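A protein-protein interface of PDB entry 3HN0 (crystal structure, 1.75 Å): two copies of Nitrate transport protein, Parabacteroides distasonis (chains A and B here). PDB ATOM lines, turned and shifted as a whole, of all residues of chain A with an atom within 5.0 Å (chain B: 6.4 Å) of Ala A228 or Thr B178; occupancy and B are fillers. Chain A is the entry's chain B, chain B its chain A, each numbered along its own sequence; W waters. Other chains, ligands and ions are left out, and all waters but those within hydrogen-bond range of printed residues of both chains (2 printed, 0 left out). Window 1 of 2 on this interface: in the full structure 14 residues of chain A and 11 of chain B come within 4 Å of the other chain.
Among the printed residues, pairs that only touch across the chains: Phe A153 with Asp B175 (3.3 Å), Phe A227 with Thr B178 (3.4 Å) and Pro A152 with Thr B178 (3.8 Å).
Water W2 lies within hydrogen-bond range of the side-chain hydroxyl (OG1) of Thr B178, the backbone carbonyl oxygen (O) of Ile A226 and the backbone carbonyl oxygen (O) of Asn B176.
Water W1 bridges OD1 of Asp B177 and O of Ile A226.
OG1 of Thr B178 lies within hydrogen-bond range of N of Ala A228.
Of the 11 printed residues of chain A, 4 touch a printed residue of chain B.
Hydrophobic or aromatic side chains of chain A within 4 Å of the printed part of chain B: Pro A152, Phe A153, Phe A227 and Ala A228.
Among the printed residues, 4 pairs touch across the chains.
Among the printed residues, no Asp or Glu carboxylate lies within 4 Å of a Lys or Arg side-chain nitrogen of the other chain.
No position is printed for both chains.
Of the 4 pairs that touch across the chains among the printed residues, none has its exchanged pair printed and touching as well.
Printed residues of chain B within 4 Å of Ala A228: Thr B178.
Thr B178 touches three residues of chain A.
Of the printed residues of chain B, Phe A227 touches Thr B178 (3.4 Å).
Printed residues of chain B within 4 Å of Phe A153: Asp B175.
Of the printed residues of chain A, Asp B175 touches Phe A153.
Of the printed residues of chain B, Pro A152 touches Thr B178.
Trp B83 touches none of the printed residues of chain A.
The nearest residue of chain B that does not touch Ala A228 is Leu B179 (4.3 Å).
The nearest residue of chain A that does not touch Thr B178 is Ile A226 (4.1 Å).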
ATOM      1  N   PRO A 152     -21.781 -22.403  14.120  1.00  0.00           N
ATOM      2  CA  PRO A 152     -20.918 -21.608  13.243  1.00  0.00           C
ATOM      3  C   PRO A 152     -21.528 -20.295  12.713  1.00  0.00           C
ATOM      4  O   PRO A 152     -20.835 -19.493  12.105  1.00  0.00           O
ATOM      5  CB  PRO A 152     -20.665 -22.565  12.058  1.00  0.00           C
ATOM      6  CG  PRO A 152     -21.846 -23.385  12.012  1.00  0.00           C
ATOM      7  CD  PRO A 152     -22.316 -23.592  13.423  1.00  0.00           C
ATOM      8  N   PHE A 153     -22.789 -20.054  12.999  1.00  0.00           N
ATOM      9  CA  PHE A 153     -23.498 -18.936  12.375  1.00  0.00           C
ATOM     10  C   PHE A 153     -22.928 -17.606  12.824  1.00  0.00           C
ATOM     11  O   PHE A 153     -22.917 -16.646  12.081  1.00  0.00           O
ATOM     12  CB  PHE A 153     -24.973 -19.048  12.709  1.00  0.00           C
ATOM     13  CG  PHE A 153     -25.574 -20.369  12.313  1.00  0.00           C
ATOM     14  CD1 PHE A 153     -25.794 -20.667  10.972  1.00  0.00           C
ATOM     15  CD2 PHE A 153     -25.885 -21.328  13.278  1.00  0.00           C
ATOM     16  CE1 PHE A 153     -26.329 -21.896  10.592  1.00  0.00           C
ATOM     17  CE2 PHE A 153     -26.431 -22.572  12.907  1.00  0.00           C
ATOM     18  CZ  PHE A 153     -26.650 -22.852  11.566  1.00  0.00           C
ATOM     19  N   ILE A 156     -20.036 -16.930  10.596  1.00  0.00           N
ATOM     20  CA  ILE A 156     -20.524 -16.672   9.228  1.00  0.00           C
ATOM     21  C   ILE A 156     -21.069 -15.245   9.154  1.00  0.00           C
ATOM     22  O   ILE A 156     -20.784 -14.518   8.200  1.00  0.00           O
ATOM     23  CB  ILE A 156     -21.630 -17.669   8.804  1.00  0.00           C
ATOM     24  CG1 ILE A 156     -21.045 -19.070   8.555  1.00  0.00           C
ATOM     25  CG2 ILE A 156     -22.338 -17.199   7.508  1.00  0.00           C
ATOM     26  CD1 ILE A 156     -22.075 -20.197   8.518  1.00  0.00           C
ATOM     27  N   GLU A 222     -13.443 -29.233   6.735  1.00  0.00           N
ATOM     28  CA  GLU A 222     -13.839 -28.773   5.412  1.00  0.00           C
ATOM     29  C   GLU A 222     -13.700 -29.866   4.380  1.00  0.00           C
ATOM     30  O   GLU A 222     -14.611 -30.061   3.569  1.00  0.00           O
ATOM     31  CB  GLU A 222     -13.065 -27.497   5.006  1.00  0.00           C
ATOM     32  CG  GLU A 222     -13.452 -26.309   5.908  1.00  0.00           C
ATOM     33  CD  GLU A 222     -12.570 -25.063   5.729  1.00  0.00           C
ATOM     34  OE1 GLU A 222     -11.521 -25.171   5.104  1.00  0.00           O
ATOM     35  OE2 GLU A 222     -12.951 -23.991   6.248  1.00  0.00           O
ATOM     36  N   ILE A 226     -17.935 -31.413   6.606  1.00  0.00           N
ATOM     37  CA  ILE A 226     -18.732 -31.203   7.845  1.00  0.00           C
ATOM     38  C   ILE A 226     -19.180 -29.758   7.980  1.00  0.00           C
ATOM     39  O   ILE A 226     -20.327 -29.432   8.376  1.00  0.00           O
ATOM     40  CB  ILE A 226     -17.929 -31.657   9.102  1.00  0.00           C
ATOM     41  CG1 ILE A 226     -17.383 -33.088   8.966  1.00  0.00           C
ATOM     42  CG2 ILE A 226     -18.791 -31.485  10.367  1.00  0.00           C
ATOM     43  CD1 ILE A 226     -18.415 -34.151   8.516  1.00  0.00           C
ATOM     44  N   PHE A 227     -18.269 -28.839   7.630  1.00  0.00           N
ATOM     45  CA  PHE A 227     -18.579 -27.455   7.587  1.00  0.00           C
ATOM     46  C   PHE A 227     -18.216 -26.927   6.239  1.00  0.00           C
ATOM     47  O   PHE A 227     -17.232 -27.421   5.655  1.00  0.00           O
ATOM     48  CB  PHE A 227     -17.804 -26.705   8.654  1.00  0.00           C
ATOM     49  CG  PHE A 227     -18.265 -27.016  10.060  1.00  0.00           C
ATOM     50  CD1 PHE A 227     -19.358 -26.345  10.600  1.00  0.00           C
ATOM     51  CD2 PHE A 227     -17.621 -27.960  10.824  1.00  0.00           C
ATOM     52  CE1 PHE A 227     -19.783 -26.635  11.904  1.00  0.00           C
ATOM     53  CE2 PHE A 227     -18.073 -28.242  12.141  1.00  0.00           C
ATOM     54  CZ  PHE A 227     -19.140 -27.571  12.640  1.00  0.00           C
ATOM     55  N   ALA A 228     -18.978 -25.931   5.792  1.00  0.00           N
ATOM     56  CA  ALA A 228     -18.670 -25.167   4.607  1.00  0.00           C
ATOM     57  C   ALA A 228     -17.307 -24.518   4.773  1.00  0.00           C
ATOM     58  O   ALA A 228     -16.952 -24.039   5.861  1.00  0.00           O
ATOM     59  CB  ALA A 228     -19.751 -24.084   4.296  1.00  0.00           C
ATOM     60  N   GLN A 229     -16.573 -24.463   3.672  1.00  0.00           N
ATOM     61  CA  GLN A 229     -15.312 -23.798   3.631  1.00  0.00           C
ATOM     62  C   GLN A 229     -15.474 -22.366   4.106  1.00  0.00           C
ATOM     63  O   GLN A 229     -16.364 -21.647   3.665  1.00  0.00           O
ATOM     64  CB  GLN A 229     -14.727 -23.819   2.220  1.00  0.00           C
ATOM     65  CG  GLN A 229     -13.317 -23.264   2.112  1.00  0.00           C
ATOM     66  CD  GLN A 229     -13.285 -21.773   1.912  1.00  0.00           C
ATOM     67  OE1 GLN A 229     -14.061 -21.222   1.136  1.00  0.00           O
ATOM     68  NE2 GLN A 229     -12.396 -21.100   2.645  1.00  0.00           N
ATOM     69  N   GLY A 230     -14.598 -21.989   5.023  1.00  0.00           N
ATOM     70  CA  GLY A 230     -14.533 -20.634   5.533  1.00  0.00           C
ATOM     71  C   GLY A 230     -15.496 -20.318   6.653  1.00  0.00           C
ATOM     72  O   GLY A 230     -15.414 -19.232   7.209  1.00  0.00           O
ATOM     73  N   ALA A 231     -16.439 -21.210   6.934  1.00  0.00           N
ATOM     74  CA  ALA A 231     -17.355 -21.019   8.062  1.00  0.00           C
ATOM     75  C   ALA A 231     -16.539 -20.800   9.317  1.00  0.00           C
ATOM     76  O   ALA A 231     -16.648 -19.733   9.944  1.00  0.00           O
ATOM     77  CB  ALA A 231     -18.244 -22.195   8.256  1.00  0.00           C
ATOM     78  N   LEU A 232     -15.684 -21.779   9.645  1.00  0.00           N
ATOM     79  CA  LEU A 232     -14.940 -21.728  10.905  1.00  0.00           C
ATOM     80  C   LEU A 232     -13.601 -21.089  10.718  1.00  0.00           C
ATOM     81  O   LEU A 232     -12.971 -21.257   9.680  1.00  0.00           O
ATOM     82  CB  LEU A 232     -14.698 -23.129  11.444  1.00  0.00           C
ATOM     83  CG  LEU A 232     -15.938 -23.936  11.806  1.00  0.00           C
ATOM     84  CD1 LEU A 232     -15.512 -25.357  12.164  1.00  0.00           C
ATOM     85  CD2 LEU A 232     -16.718 -23.323  12.951  1.00  0.00           C
ATOM     86  N   TRP B  83     -21.561 -25.055  -4.469  1.00  0.00           N
ATOM     87  CA  TRP B  83     -22.511 -25.393  -3.415  1.00  0.00           C
ATOM     88  C   TRP B  83     -23.626 -24.330  -3.233  1.00  0.00           C
ATOM     89  O   TRP B  83     -24.537 -24.502  -2.442  1.00  0.00           O
ATOM     90  CB  TRP B  83     -21.742 -25.633  -2.090  1.00  0.00           C
ATOM     91  CG  TRP B  83     -20.764 -26.776  -2.271  1.00  0.00           C
ATOM     92  CD1 TRP B  83     -19.508 -26.691  -2.773  1.00  0.00           C
ATOM     93  CD2 TRP B  83     -21.043 -28.179  -2.097  1.00  0.00           C
ATOM     94  NE1 TRP B  83     -18.952 -27.936  -2.900  1.00  0.00           N
ATOM     95  CE2 TRP B  83     -19.857 -28.878  -2.453  1.00  0.00           C
ATOM     96  CE3 TRP B  83     -22.146 -28.906  -1.619  1.00  0.00           C
ATOM     97  CZ2 TRP B  83     -19.758 -30.242  -2.403  1.00  0.00           C
ATOM     98  CZ3 TRP B  83     -22.038 -30.289  -1.538  1.00  0.00           C
ATOM     99  CH2 TRP B  83     -20.844 -30.953  -1.955  1.00  0.00           C
ATOM    100  N   HIS B 172     -29.703 -25.637   1.374  1.00  0.00           N
ATOM    101  CA  HIS B 172     -29.412 -26.477   2.532  1.00  0.00           C
ATOM    102  C   HIS B 172     -30.548 -27.400   2.879  1.00  0.00           C
ATOM    103  O   HIS B 172     -31.713 -27.016   2.833  1.00  0.00           O
ATOM    104  CB  HIS B 172     -29.059 -25.612   3.755  1.00  0.00           C
ATOM    105  CG  HIS B 172     -28.023 -24.579   3.489  1.00  0.00           C
ATOM    106  ND1 HIS B 172     -26.669 -24.841   3.538  1.00  0.00           N
ATOM    107  CD2 HIS B 172     -28.144 -23.264   3.204  1.00  0.00           C
ATOM    108  CE1 HIS B 172     -26.002 -23.727   3.270  1.00  0.00           C
ATOM    109  NE2 HIS B 172     -26.874 -22.761   3.050  1.00  0.00           N
ATOM    110  N   THR B 174     -31.092 -28.623   6.001  1.00  0.00           N
ATOM    111  CA  THR B 174     -31.510 -28.215   7.333  1.00  0.00           C
ATOM    112  C   THR B 174     -30.652 -27.033   7.705  1.00  0.00           C
ATOM    113  O   THR B 174     -29.662 -26.746   7.014  1.00  0.00           O
ATOM    114  CB  THR B 174     -31.210 -29.382   8.366  1.00  0.00           C
ATOM    115  OG1 THR B 174     -29.790 -29.693   8.394  1.00  0.00           O
ATOM    116  CG2 THR B 174     -31.974 -30.650   7.998  1.00  0.00           C
ATOM    117  N   ASP B 175     -30.946 -26.371   8.821  1.00  0.00           N
ATOM    118  CA  ASP B 175     -30.021 -25.334   9.345  1.00  0.00           C
ATOM    119  C   ASP B 175     -28.629 -25.795   9.772  1.00  0.00           C
ATOM    120  O   ASP B 175     -27.633 -25.166   9.403  1.00  0.00           O
ATOM    121  CB  ASP B 175     -30.688 -24.572  10.464  1.00  0.00           C
ATOM    122  CG  ASP B 175     -31.632 -23.557   9.929  1.00  0.00           C
ATOM    123  OD1 ASP B 175     -31.112 -22.583   9.326  1.00  0.00           O
ATOM    124  OD2 ASP B 175     -32.861 -23.773  10.053  1.00  0.00           O
ATOM    125  N   ASN B 176     -28.512 -26.891  10.514  1.00  0.00           N
ATOM    126  CA  ASN B 176     -27.158 -27.410  10.808  1.00  0.00           C
ATOM    127  C   ASN B 176     -26.357 -27.863   9.554  1.00  0.00           C
ATOM    128  O   ASN B 176     -25.193 -28.252   9.680  1.00  0.00           O
ATOM    129  CB  ASN B 176     -27.186 -28.518  11.892  1.00  0.00           C
ATOM    130  N   ASP B 177     -26.935 -27.771   8.352  1.00  0.00           N
ATOM    131  CA  ASP B 177     -26.272 -28.238   7.136  1.00  0.00           C
ATOM    132  C   ASP B 177     -25.609 -27.004   6.505  1.00  0.00           C
ATOM    133  O   ASP B 177     -26.159 -26.487   5.561  1.00  0.00           O
ATOM    134  CB  ASP B 177     -27.314 -28.904   6.174  1.00  0.00           C
ATOM    135  CG  ASP B 177     -26.676 -29.508   4.835  1.00  0.00           C
ATOM    136  OD1 ASP B 177     -25.525 -29.924   4.959  1.00  0.00           O
ATOM    137  OD2 ASP B 177     -27.296 -29.559   3.675  1.00  0.00           O
ATOM    138  N   THR B 178     -24.441 -26.527   6.993  1.00  0.00           N
ATOM    139  CA  THR B 178     -23.751 -25.401   6.320  1.00  0.00           C
ATOM    140  C   THR B 178     -23.232 -25.794   4.949  1.00  0.00           C
ATOM    141  O   THR B 178     -23.006 -24.915   4.114  1.00  0.00           O
ATOM    142  CB  THR B 178     -22.541 -24.745   7.123  1.00  0.00           C
ATOM    143  OG1 THR B 178     -21.473 -25.679   7.276  1.00  0.00           O
ATOM    144  CG2 THR B 178     -23.005 -24.248   8.479  1.00  0.00           C
ATOM    145  N   LEU B 179     -23.015 -27.080   4.712  1.00  0.00           N
ATOM    146  CA  LEU B 179     -22.470 -27.520   3.413  1.00  0.00           C
ATOM    147  C   LEU B 179     -23.513 -27.352   2.313  1.00  0.00           C
ATOM    148  O   LEU B 179     -23.215 -26.816   1.248  1.00  0.00           O
ATOM    149  CB  LEU B 179     -21.987 -28.982   3.440  1.00  0.00           C
ATOM    150  CG  LEU B 179     -21.464 -29.559   2.114  1.00  0.00           C
ATOM    151  CD1 LEU B 179     -20.256 -28.799   1.660  1.00  0.00           C
ATOM    152  CD2 LEU B 179     -21.130 -31.082   2.151  1.00  0.00           C
ATOM    153  N   GLY B 180     -24.736 -27.765   2.580  1.00  0.00           N
ATOM    154  CA  GLY B 180     -25.742 -27.770   1.502  1.00  0.00           C
ATOM    155  C   GLY B 180     -25.624 -28.848   0.450  1.00  0.00           C
ATOM    156  O   GLY B 180     -24.772 -29.734   0.507  1.00  0.00           O
ATOM    157  N   LYS B 241     -20.384 -20.244  -3.491  1.00  0.00           N
ATOM    158  CA  LYS B 241     -19.865 -21.242  -2.522  1.00  0.00           C
ATOM    159  C   LYS B 241     -18.999 -22.297  -3.261  1.00  0.00           C
ATOM    160  O   LYS B 241     -19.280 -23.512  -3.251  1.00  0.00           O
ATOM    161  CB  LYS B 241     -21.008 -21.941  -1.755  1.00  0.00           C
ATOM    162  CG  LYS B 241     -21.915 -20.976  -0.915  1.00  0.00           C
ATOM    163  CD  LYS B 241     -21.120 -20.267   0.184  1.00  0.00           C
ATOM    164  CE  LYS B 241     -21.991 -19.324   1.054  1.00  0.00           C
ATOM    165  NZ  LYS B 241     -22.044 -17.949   0.484  1.00  0.00           N
HETATM  166  O   HOH W   1     -23.112 -30.022   6.638  1.00  0.00           O
HETATM  167  O   HOH W   2     -22.224 -27.582   8.935  1.00  0.00           O
